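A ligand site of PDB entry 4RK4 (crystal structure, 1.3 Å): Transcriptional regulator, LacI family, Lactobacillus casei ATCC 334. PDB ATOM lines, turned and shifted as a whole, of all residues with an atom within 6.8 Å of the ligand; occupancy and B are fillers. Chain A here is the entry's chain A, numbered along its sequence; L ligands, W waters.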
ATOM      1  N   SER A  17     -23.948  11.345 -16.328  1.00  0.00           N
ATOM      2  CA  SER A  17     -24.236  11.453 -17.770  1.00  0.00           C
ATOM      3  C   SER A  17     -25.508  10.659 -18.116  1.00  0.00           C
ATOM      4  O   SER A  17     -26.313  11.137 -18.939  1.00  0.00           O
ATOM      5  CB  SER A  17     -23.112  11.091 -18.599  1.00  0.00           C
ATOM      6  OG  SER A  17     -22.706   9.853 -18.445  1.00  0.00           O
ATOM      7  N   ARG A  18     -25.704   9.487 -17.542  1.00  0.00           N
ATOM      8  CA  ARG A  18     -26.806   8.596 -17.950  1.00  0.00           C
ATOM      9  C   ARG A  18     -27.146   7.650 -16.839  1.00  0.00           C
ATOM     10  O   ARG A  18     -26.307   6.855 -16.394  1.00  0.00           O
ATOM     11  CB  ARG A  18     -26.413   7.827 -19.169  1.00  0.00           C
ATOM     12  CG  ARG A  18     -27.503   6.953 -19.741  1.00  0.00           C
ATOM     13  CD  ARG A  18     -27.199   6.425 -21.156  1.00  0.00           C
ATOM     14  NE  ARG A  18     -25.944   5.729 -21.247  1.00  0.00           N
ATOM     15  CZ  ARG A  18     -25.719   4.421 -20.989  1.00  0.00           C
ATOM     16  NH1 ARG A  18     -26.658   3.581 -20.737  1.00  0.00           N
ATOM     17  NH2 ARG A  18     -24.438   4.058 -21.082  1.00  0.00           N
ATOM     18  N   ASN A  21     -26.828   3.819 -17.306  1.00  0.00           N
ATOM     19  CA  ASN A  21     -25.492   3.201 -17.144  1.00  0.00           C
ATOM     20  C   ASN A  21     -25.462   2.594 -15.727  1.00  0.00           C
ATOM     21  O   ASN A  21     -25.533   3.354 -14.763  1.00  0.00           O
ATOM     22  CB  ASN A  21     -24.441   4.256 -17.326  1.00  0.00           C
ATOM     23  CG  ASN A  21     -23.034   3.731 -17.130  1.00  0.00           C
ATOM     24  OD1 ASN A  21     -22.828   2.710 -16.494  1.00  0.00           O
ATOM     25  ND2 ASN A  21     -22.077   4.469 -17.613  1.00  0.00           N
ATOM     26  N   PRO A  22     -25.401   1.261 -15.583  1.00  0.00           N
ATOM     27  CA  PRO A  22     -25.493   0.692 -14.246  1.00  0.00           C
ATOM     28  C   PRO A  22     -24.389   1.151 -13.318  1.00  0.00           C
ATOM     29  O   PRO A  22     -24.584   1.047 -12.092  1.00  0.00           O
ATOM     30  CB  PRO A  22     -25.430  -0.812 -14.509  1.00  0.00           C
ATOM     31  CG  PRO A  22     -25.956  -0.920 -15.901  1.00  0.00           C
ATOM     32  CD  PRO A  22     -25.422   0.222 -16.630  1.00  0.00           C
ATOM     33  N   PHE A  23     -23.252   1.584 -13.813  1.00  0.00           N
ATOM     34  CA  PHE A  23     -22.242   2.178 -12.982  1.00  0.00           C
ATOM     35  C   PHE A  23     -22.807   3.400 -12.263  1.00  0.00           C
ATOM     36  O   PHE A  23     -22.651   3.569 -11.035  1.00  0.00           O
ATOM     37  CB  PHE A  23     -21.003   2.525 -13.790  1.00  0.00           C
ATOM     38  CG  PHE A  23     -20.009   3.364 -13.005  1.00  0.00           C
ATOM     39  CD1 PHE A  23     -19.235   2.771 -11.979  1.00  0.00           C
ATOM     40  CD2 PHE A  23     -19.943   4.705 -13.170  1.00  0.00           C
ATOM     41  CE1 PHE A  23     -18.438   3.539 -11.208  1.00  0.00           C
ATOM     42  CE2 PHE A  23     -19.132   5.479 -12.374  1.00  0.00           C
ATOM     43  CZ  PHE A  23     -18.379   4.873 -11.375  1.00  0.00           C
ATOM     44  N   PHE A  24     -23.417   4.304 -13.011  1.00  0.00           N
ATOM     45  CA  PHE A  24     -23.970   5.510 -12.405  1.00  0.00           C
ATOM     46  C   PHE A  24     -25.130   5.214 -11.515  1.00  0.00           C
ATOM     47  O   PHE A  24     -25.305   5.845 -10.470  1.00  0.00           O
ATOM     48  CB  PHE A  24     -24.344   6.556 -13.446  1.00  0.00           C
ATOM     49  CG  PHE A  24     -23.162   7.255 -14.065  1.00  0.00           C
ATOM     50  CD1 PHE A  24     -22.201   7.873 -13.278  1.00  0.00           C
ATOM     51  CD2 PHE A  24     -23.038   7.345 -15.413  1.00  0.00           C
ATOM     52  CE1 PHE A  24     -21.153   8.577 -13.850  1.00  0.00           C
ATOM     53  CE2 PHE A  24     -21.975   8.045 -15.977  1.00  0.00           C
ATOM     54  CZ  PHE A  24     -21.028   8.623 -15.162  1.00  0.00           C
ATOM     55  N   ALA A  72     -20.553  13.303 -10.757  1.00  0.00           N
ATOM     56  CA  ALA A  72     -19.801  12.145 -11.209  1.00  0.00           C
ATOM     57  C   ALA A  72     -19.438  12.209 -12.688  1.00  0.00           C
ATOM     58  O   ALA A  72     -18.809  11.316 -13.219  1.00  0.00           O
ATOM     59  CB  ALA A  72     -20.487  10.842 -10.870  1.00  0.00           C
ATOM     60  N   SER A  73     -19.857  13.296 -13.338  1.00  0.00           N
ATOM     61  CA  SER A  73     -19.588  13.637 -14.732  1.00  0.00           C
ATOM     62  C   SER A  73     -19.400  15.143 -14.751  1.00  0.00           C
ATOM     63  O   SER A  73     -20.154  15.820 -14.129  1.00  0.00           O
ATOM     64  CB  SER A  73     -20.812  13.170 -15.618  1.00  0.00           C
ATOM     65  OG  SER A  73     -21.035  11.758 -15.628  1.00  0.00           O
ATOM     66  N   VAL A  94     -16.560  13.501  -8.111  1.00  0.00           N
ATOM     67  CA  VAL A  94     -16.060  12.142  -7.897  1.00  0.00           C
ATOM     68  C   VAL A  94     -15.909  11.398  -9.221  1.00  0.00           C
ATOM     69  O   VAL A  94     -16.837  11.283  -9.999  1.00  0.00           O
ATOM     70  CB  VAL A  94     -16.904  11.340  -6.905  1.00  0.00           C
ATOM     71  CG1 VAL A  94     -18.352  11.213  -7.338  1.00  0.00           C
ATOM     72  CG2 VAL A  94     -16.304   9.976  -6.599  1.00  0.00           C
ATOM     73  N   ASN A  95     -14.720  10.888  -9.465  1.00  0.00           N
ATOM     74  CA  ASN A  95     -14.452   9.975 -10.544  1.00  0.00           C
ATOM     75  C   ASN A  95     -14.693  10.553 -11.925  1.00  0.00           C
ATOM     76  O   ASN A  95     -15.052   9.818 -12.820  1.00  0.00           O
ATOM     77  CB  ASN A  95     -15.218   8.662 -10.357  1.00  0.00           C
ATOM     78  CG  ASN A  95     -14.633   7.514 -11.135  1.00  0.00           C
ATOM     79  OD1 ASN A  95     -13.431   7.412 -11.257  1.00  0.00           O
ATOM     80  ND2 ASN A  95     -15.488   6.635 -11.595  1.00  0.00           N
ATOM     81  N   ALA A  96     -14.428  11.846 -12.080  1.00  0.00           N
ATOM     82  CA  ALA A  96     -14.605  12.534 -13.335  1.00  0.00           C
ATOM     83  C   ALA A  96     -13.300  12.843 -14.019  1.00  0.00           C
ATOM     84  O   ALA A  96     -13.325  13.597 -15.026  1.00  0.00           O
ATOM     85  CB  ALA A  96     -15.460  13.801 -13.129  1.00  0.00           C
ATOM     86  N   HIS A 110      -7.366   5.725 -13.469  1.00  0.00           N
ATOM     87  CA  HIS A 110      -7.807   4.993 -14.671  1.00  0.00           C
ATOM     88  C   HIS A 110      -6.744   4.778 -15.689  1.00  0.00           C
ATOM     89  O   HIS A 110      -6.732   3.787 -16.387  1.00  0.00           O
ATOM     90  CB  HIS A 110      -9.030   5.703 -15.291  1.00  0.00           C
ATOM     91  CG  HIS A 110     -10.235   5.612 -14.462  1.00  0.00           C
ATOM     92  ND1 HIS A 110     -10.968   4.467 -14.340  1.00  0.00           N
ATOM     93  CD2 HIS A 110     -10.811   6.516 -13.660  1.00  0.00           C
ATOM     94  CE1 HIS A 110     -11.963   4.664 -13.512  1.00  0.00           C
ATOM     95  NE2 HIS A 110     -11.910   5.925 -13.087  1.00  0.00           N
ATOM     96  N   HIS A 142     -14.473  12.422 -22.485  1.00  0.00           N
ATOM     97  CA  HIS A 142     -14.615  11.612 -21.293  1.00  0.00           C
ATOM     98  C   HIS A 142     -13.803  10.351 -21.592  1.00  0.00           C
ATOM     99  O   HIS A 142     -13.968   9.668 -22.663  1.00  0.00           O
ATOM    100  CB  HIS A 142     -16.071  11.214 -20.951  1.00  0.00           C
ATOM    101  CG  HIS A 142     -16.937  12.355 -20.536  1.00  0.00           C
ATOM    102  ND1 HIS A 142     -16.639  13.132 -19.453  1.00  0.00           N
ATOM    103  CD2 HIS A 142     -18.037  12.901 -21.103  1.00  0.00           C
ATOM    104  CE1 HIS A 142     -17.556  14.083 -19.313  1.00  0.00           C
ATOM    105  NE2 HIS A 142     -18.402  13.974 -20.304  1.00  0.00           N
ATOM    106  N   GLY A 143     -12.961  10.024 -20.628  1.00  0.00           N
ATOM    107  CA  GLY A 143     -12.204   8.785 -20.747  1.00  0.00           C
ATOM    108  C   GLY A 143     -10.885   8.958 -21.472  1.00  0.00           C
ATOM    109  O   GLY A 143     -10.297   7.997 -21.868  1.00  0.00           O
ATOM    110  N   ARG A 146      -7.801   7.040 -20.270  1.00  0.00           N
ATOM    111  CA  ARG A 146      -7.812   5.674 -20.778  1.00  0.00           C
ATOM    112  C   ARG A 146      -7.307   5.611 -22.201  1.00  0.00           C
ATOM    113  O   ARG A 146      -6.542   4.716 -22.585  1.00  0.00           O
ATOM    114  CB  ARG A 146      -9.171   5.042 -20.655  1.00  0.00           C
ATOM    115  CG  ARG A 146      -9.727   5.148 -19.247  1.00  0.00           C
ATOM    116  CD  ARG A 146     -11.081   4.635 -19.218  1.00  0.00           C
ATOM    117  NE  ARG A 146     -11.746   4.942 -18.000  1.00  0.00           N
ATOM    118  CZ  ARG A 146     -12.977   4.461 -17.757  1.00  0.00           C
ATOM    119  NH1 ARG A 146     -13.583   3.593 -18.602  1.00  0.00           N
ATOM    120  NH2 ARG A 146     -13.581   4.808 -16.664  1.00  0.00           N
ATOM    121  N   HIS A 171     -21.567   3.625 -26.310  1.00  0.00           N
ATOM    122  CA  HIS A 171     -21.995   3.682 -24.933  1.00  0.00           C
ATOM    123  C   HIS A 171     -22.772   2.525 -24.441  1.00  0.00           C
ATOM    124  O   HIS A 171     -22.656   2.092 -23.302  1.00  0.00           O
ATOM    125  CB  HIS A 171     -22.857   4.959 -24.734  1.00  0.00           C
ATOM    126  CG  HIS A 171     -22.193   6.210 -25.156  1.00  0.00           C
ATOM    127  ND1 HIS A 171     -22.572   6.934 -26.245  1.00  0.00           N
ATOM    128  CD2 HIS A 171     -21.165   6.858 -24.605  1.00  0.00           C
ATOM    129  CE1 HIS A 171     -21.754   7.959 -26.370  1.00  0.00           C
ATOM    130  NE2 HIS A 171     -20.893   7.952 -25.391  1.00  0.00           N
ATOM    131  N   ASN A 198     -14.109  -0.384 -22.728  1.00  0.00           N
ATOM    132  CA  ASN A 198     -14.375   0.754 -21.863  1.00  0.00           C
ATOM    133  C   ASN A 198     -15.731   0.705 -21.165  1.00  0.00           C
ATOM    134  O   ASN A 198     -16.098   1.704 -20.533  1.00  0.00           O
ATOM    135  CB  ASN A 198     -14.146   2.096 -22.587  1.00  0.00           C
ATOM    136  CG  ASN A 198     -12.797   2.676 -22.333  1.00  0.00           C
ATOM    137  OD1 ASN A 198     -12.372   2.732 -21.163  1.00  0.00           O
ATOM    138  ND2 ASN A 198     -12.105   3.092 -23.342  1.00  0.00           N
ATOM    139  N   SER A 199     -16.445  -0.403 -21.201  1.00  0.00           N
ATOM    140  CA  SER A 199     -17.752  -0.433 -20.572  1.00  0.00           C
ATOM    141  C   SER A 199     -18.322  -1.837 -20.583  1.00  0.00           C
ATOM    142  O   SER A 199     -18.380  -2.486 -21.643  1.00  0.00           O
ATOM    143  CB  SER A 199     -18.751   0.423 -21.376  1.00  0.00           C
ATOM    144  OG  SER A 199     -20.089   0.039 -21.169  1.00  0.00           O
ATOM    145  N   ASP A 200     -18.799  -2.295 -19.423  1.00  0.00           N
ATOM    146  CA  ASP A 200     -19.432  -3.597 -19.363  1.00  0.00           C
ATOM    147  C   ASP A 200     -20.708  -3.673 -20.186  1.00  0.00           C
ATOM    148  O   ASP A 200     -21.082  -4.748 -20.685  1.00  0.00           O
ATOM    149  CB  ASP A 200     -19.729  -4.004 -17.919  1.00  0.00           C
ATOM    150  CG  ASP A 200     -18.472  -4.374 -17.137  1.00  0.00           C
ATOM    151  OD1 ASP A 200     -17.389  -4.546 -17.712  1.00  0.00           O
ATOM    152  OD2 ASP A 200     -18.611  -4.465 -15.865  1.00  0.00           O
ATOM    153  N   GLU A 201     -21.446  -2.552 -20.293  1.00  0.00           N
ATOM    154  CA  GLU A 201     -22.624  -2.539 -21.190  1.00  0.00           C
ATOM    155  C   GLU A 201     -22.195  -2.842 -22.639  1.00  0.00           C
ATOM    156  O   GLU A 201     -22.763  -3.710 -23.303  1.00  0.00           O
ATOM    157  CB  GLU A 201     -23.321  -1.146 -21.217  1.00  0.00           C
ATOM    158  CG  GLU A 201     -23.986  -0.784 -19.945  1.00  0.00           C
ATOM    159  CD  GLU A 201     -24.542   0.636 -20.082  1.00  0.00           C
ATOM    160  OE1 GLU A 201     -23.873   1.599 -19.726  1.00  0.00           O
ATOM    161  OE2 GLU A 201     -25.716   0.823 -20.559  1.00  0.00           O
ATOM    162  N   TYR A 226     -15.327  -2.882 -18.673  1.00  0.00           N
ATOM    163  CA  TYR A 226     -14.876  -1.869 -17.696  1.00  0.00           C
ATOM    164  C   TYR A 226     -16.026  -1.592 -16.759  1.00  0.00           C
ATOM    165  O   TYR A 226     -17.137  -1.325 -17.229  1.00  0.00           O
ATOM    166  CB  TYR A 226     -14.420  -0.569 -18.385  1.00  0.00           C
ATOM    167  CG  TYR A 226     -13.292   0.175 -17.649  1.00  0.00           C
ATOM    168  CD1 TYR A 226     -13.508   0.876 -16.470  1.00  0.00           C
ATOM    169  CD2 TYR A 226     -12.018   0.158 -18.135  1.00  0.00           C
ATOM    170  CE1 TYR A 226     -12.493   1.551 -15.833  1.00  0.00           C
ATOM    171  CE2 TYR A 226     -10.998   0.872 -17.580  1.00  0.00           C
ATOM    172  CZ  TYR A 226     -11.249   1.556 -16.374  1.00  0.00           C
ATOM    173  OH  TYR A 226     -10.193   2.266 -15.789  1.00  0.00           O
ATOM    174  N   ASP A 227     -15.740  -1.644 -15.467  1.00  0.00           N
ATOM    175  CA  ASP A 227     -16.521  -1.173 -14.324  1.00  0.00           C
ATOM    176  C   ASP A 227     -16.762  -2.292 -13.312  1.00  0.00           C
ATOM    177  O   ASP A 227     -16.777  -2.001 -12.088  1.00  0.00           O
ATOM    178  CB  ASP A 227     -17.866  -0.541 -14.619  1.00  0.00           C
ATOM    179  CG  ASP A 227     -17.779   0.752 -15.413  1.00  0.00           C
ATOM    180  OD1 ASP A 227     -16.703   1.375 -15.513  1.00  0.00           O
ATOM    181  OD2 ASP A 227     -18.892   1.136 -15.913  1.00  0.00           O
ATOM    182  N   GLN A 229     -19.827  -4.012 -13.362  1.00  0.00           N
ATOM    183  CA  GLN A 229     -21.205  -3.687 -13.132  1.00  0.00           C
ATOM    184  C   GLN A 229     -21.939  -4.932 -12.567  1.00  0.00           C
ATOM    185  O   GLN A 229     -21.472  -6.058 -12.649  1.00  0.00           O
ATOM    186  CB  GLN A 229     -21.854  -3.224 -14.412  1.00  0.00           C
ATOM    187  CG  GLN A 229     -21.275  -1.880 -14.840  1.00  0.00           C
ATOM    188  CD  GLN A 229     -21.805  -1.358 -16.174  1.00  0.00           C
ATOM    189  OE1 GLN A 229     -22.770  -1.892 -16.726  1.00  0.00           O
ATOM    190  NE2 GLN A 229     -21.175  -0.348 -16.699  1.00  0.00           N
ATOM    191  N   GLN A 244     -14.388  -1.059 -10.611  1.00  0.00           N
ATOM    192  CA  GLN A 244     -14.431   0.231  -9.906  1.00  0.00           C
ATOM    193  C   GLN A 244     -15.027   0.023  -8.510  1.00  0.00           C
ATOM    194  O   GLN A 244     -16.039  -0.630  -8.390  1.00  0.00           O
ATOM    195  CB  GLN A 244     -15.240   1.277 -10.673  1.00  0.00           C
ATOM    196  CG  GLN A 244     -14.652   1.617 -12.040  1.00  0.00           C
ATOM    197  CD  GLN A 244     -14.979   3.009 -12.479  1.00  0.00           C
ATOM    198  OE1 GLN A 244     -14.630   3.958 -11.770  1.00  0.00           O
ATOM    199  NE2 GLN A 244     -15.553   3.152 -13.635  1.00  0.00           N
HETATM  200  C1  LIG L   1     -18.733   6.786 -17.501  1.00  0.00           C
HETATM  201  C2  LIG L   1     -18.030   6.786 -16.163  1.00  0.00           C
HETATM  202  C3  LIG L   1     -16.801   5.856 -16.237  1.00  0.00           C
HETATM  203  C4  LIG L   1     -17.298   4.475 -16.647  1.00  0.00           C
HETATM  204  C5  LIG L   1     -17.974   4.606 -18.010  1.00  0.00           C
HETATM  205  C6  LIG L   1     -18.559   3.321 -18.554  1.00  0.00           C
HETATM  206  O1  LIG L   1     -17.880   7.428 -18.447  1.00  0.00           O
HETATM  207  O2  LIG L   1     -17.603   8.128 -15.809  1.00  0.00           O
HETATM  208  O3  LIG L   1     -16.211   5.779 -14.937  1.00  0.00           O
HETATM  209  O4  LIG L   1     -16.191   3.590 -16.819  1.00  0.00           O
HETATM  210  O5  LIG L   1     -19.098   5.541 -17.968  1.00  0.00           O
HETATM  211  O6  LIG L   1     -19.620   2.844 -17.702  1.00  0.00           O
HETATM  212  O   HOH W   1     -21.320   1.439 -19.291  1.00  0.00           O
HETATM  213  O   HOH W   2     -19.032   7.903 -20.934  1.00  0.00           O
HETATM  214  O   HOH W   3     -17.581   8.801 -13.104  1.00  0.00           O
HETATM  215  O   HOH W   4     -16.093   4.482 -20.836  1.00  0.00           O
HETATM  216  O   HOH W   5     -19.127  10.639 -17.409  1.00  0.00           O
HETATM  217  O   HOH W   6     -14.327   7.757 -14.717  1.00  0.00           O
HETATM  218  O   HOH W   7     -15.146   7.017 -19.458  1.00  0.00           O
HETATM  219  O   HOH W   8     -17.050  11.212 -15.661  1.00  0.00           O
HETATM  220  O   HOH W   9     -15.255   9.133 -17.443  1.00  0.00           O
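The side-chain carboxylate (OD2) of Asp 227 sits at hydrogen-bond distance from an oxygen (O6) of the ligand (2.6 Å). An oxygen (O4) of the ligand sits at hydrogen-bond distance from the guanidinium group (NH2) of Arg 146 (2.9 Å). ND2 of Asn 21 lies within hydrogen-bond range of O6 of the ligand. The side-chain amide nitrogen (NE2) of Gln 244 is in hydrogen-bond range of an oxygen (O3) of the ligand.
The side-chain carboxylate (OD1) of Asp 227 is in hydrogen-bond range of the side-chain amide nitrogen (NE2) of Gln 244, at 2.8 Å. The side-chain carboxylate (OD2) of Asp 227 is in hydrogen-bond range of the side-chain amide nitrogen (NE2) of Gln 229 (2.8 Å). The side-chain amide oxygen (OD1) of Asn 198 sits at hydrogen-bond distance from the guanidinium group (NH1) of Arg 146 (3.0 Å). The side-chain amide oxygen (OD1) of Asn 21 lies within hydrogen-bond range of the backbone NH (N) of Phe 23. The side-chain amide oxygen (OE1) of Gln 244 lies within hydrogen-bond range of the side-chain amide nitrogen (ND2) of Asn 95 (2.8 Å). OD2 of Asp 200 sits at hydrogen-bond distance from N of Gln 229 (2.8 Å). OH of Tyr 226 is in hydrogen-bond range of ND1 of His 110 (2.7 Å). N of Tyr 226 lies within hydrogen-bond range of OD1 of Asp 200, at 2.8 Å.
Merely in contact with the ligand: Phe 23 (3.9 Å), Phe 24 (3.5 Å), Asn 95 (3.5 Å), Asn 198 (3.5 Å), Tyr 226 (3.8 Å) and Gln 229 (3.7 Å). Hydrophobic or aromatic side chains that line the ligand: Phe 23, Phe 24 and Tyr 226. Of the 24 residues printed, 10 come within 4 Å of the ligand. The nearest printed residue that does not touch the ligand is Ser 199 (4.05 Å).
Water W1 lies within hydrogen-bond range of OE1 of Glu 201, OG of Ser 199, O6 of the ligand, NE2 of Gln 229 and OD1 of Asn 21. Water W6 lies within hydrogen-bond range of an oxygen (O3) of the ligand (2.7 Å), the backbone carbonyl oxygen (O) of Asn 95 (2.9 Å) and a ring nitrogen (NE2) of His 110 (3.4 Å). Water W3 lies within hydrogen-bond range of the backbone carbonyl oxygen (O) of Asn 95, an oxygen (O2) of the ligand and the backbone carbonyl oxygen (O) of Ala 72. Water W8 bridges the backbone carbonyl oxygen of Ala 72 (3.0 Å) and an oxygen (O2) of the ligand (3.1 Å). Water W5 lies within hydrogen-bond range of OG of Ser 73 and O2 of the ligand. Water W4 bridges the backbone carbonyl oxygen (O) of Asn 198 and the guanidinium group (NH1) of Arg 146.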
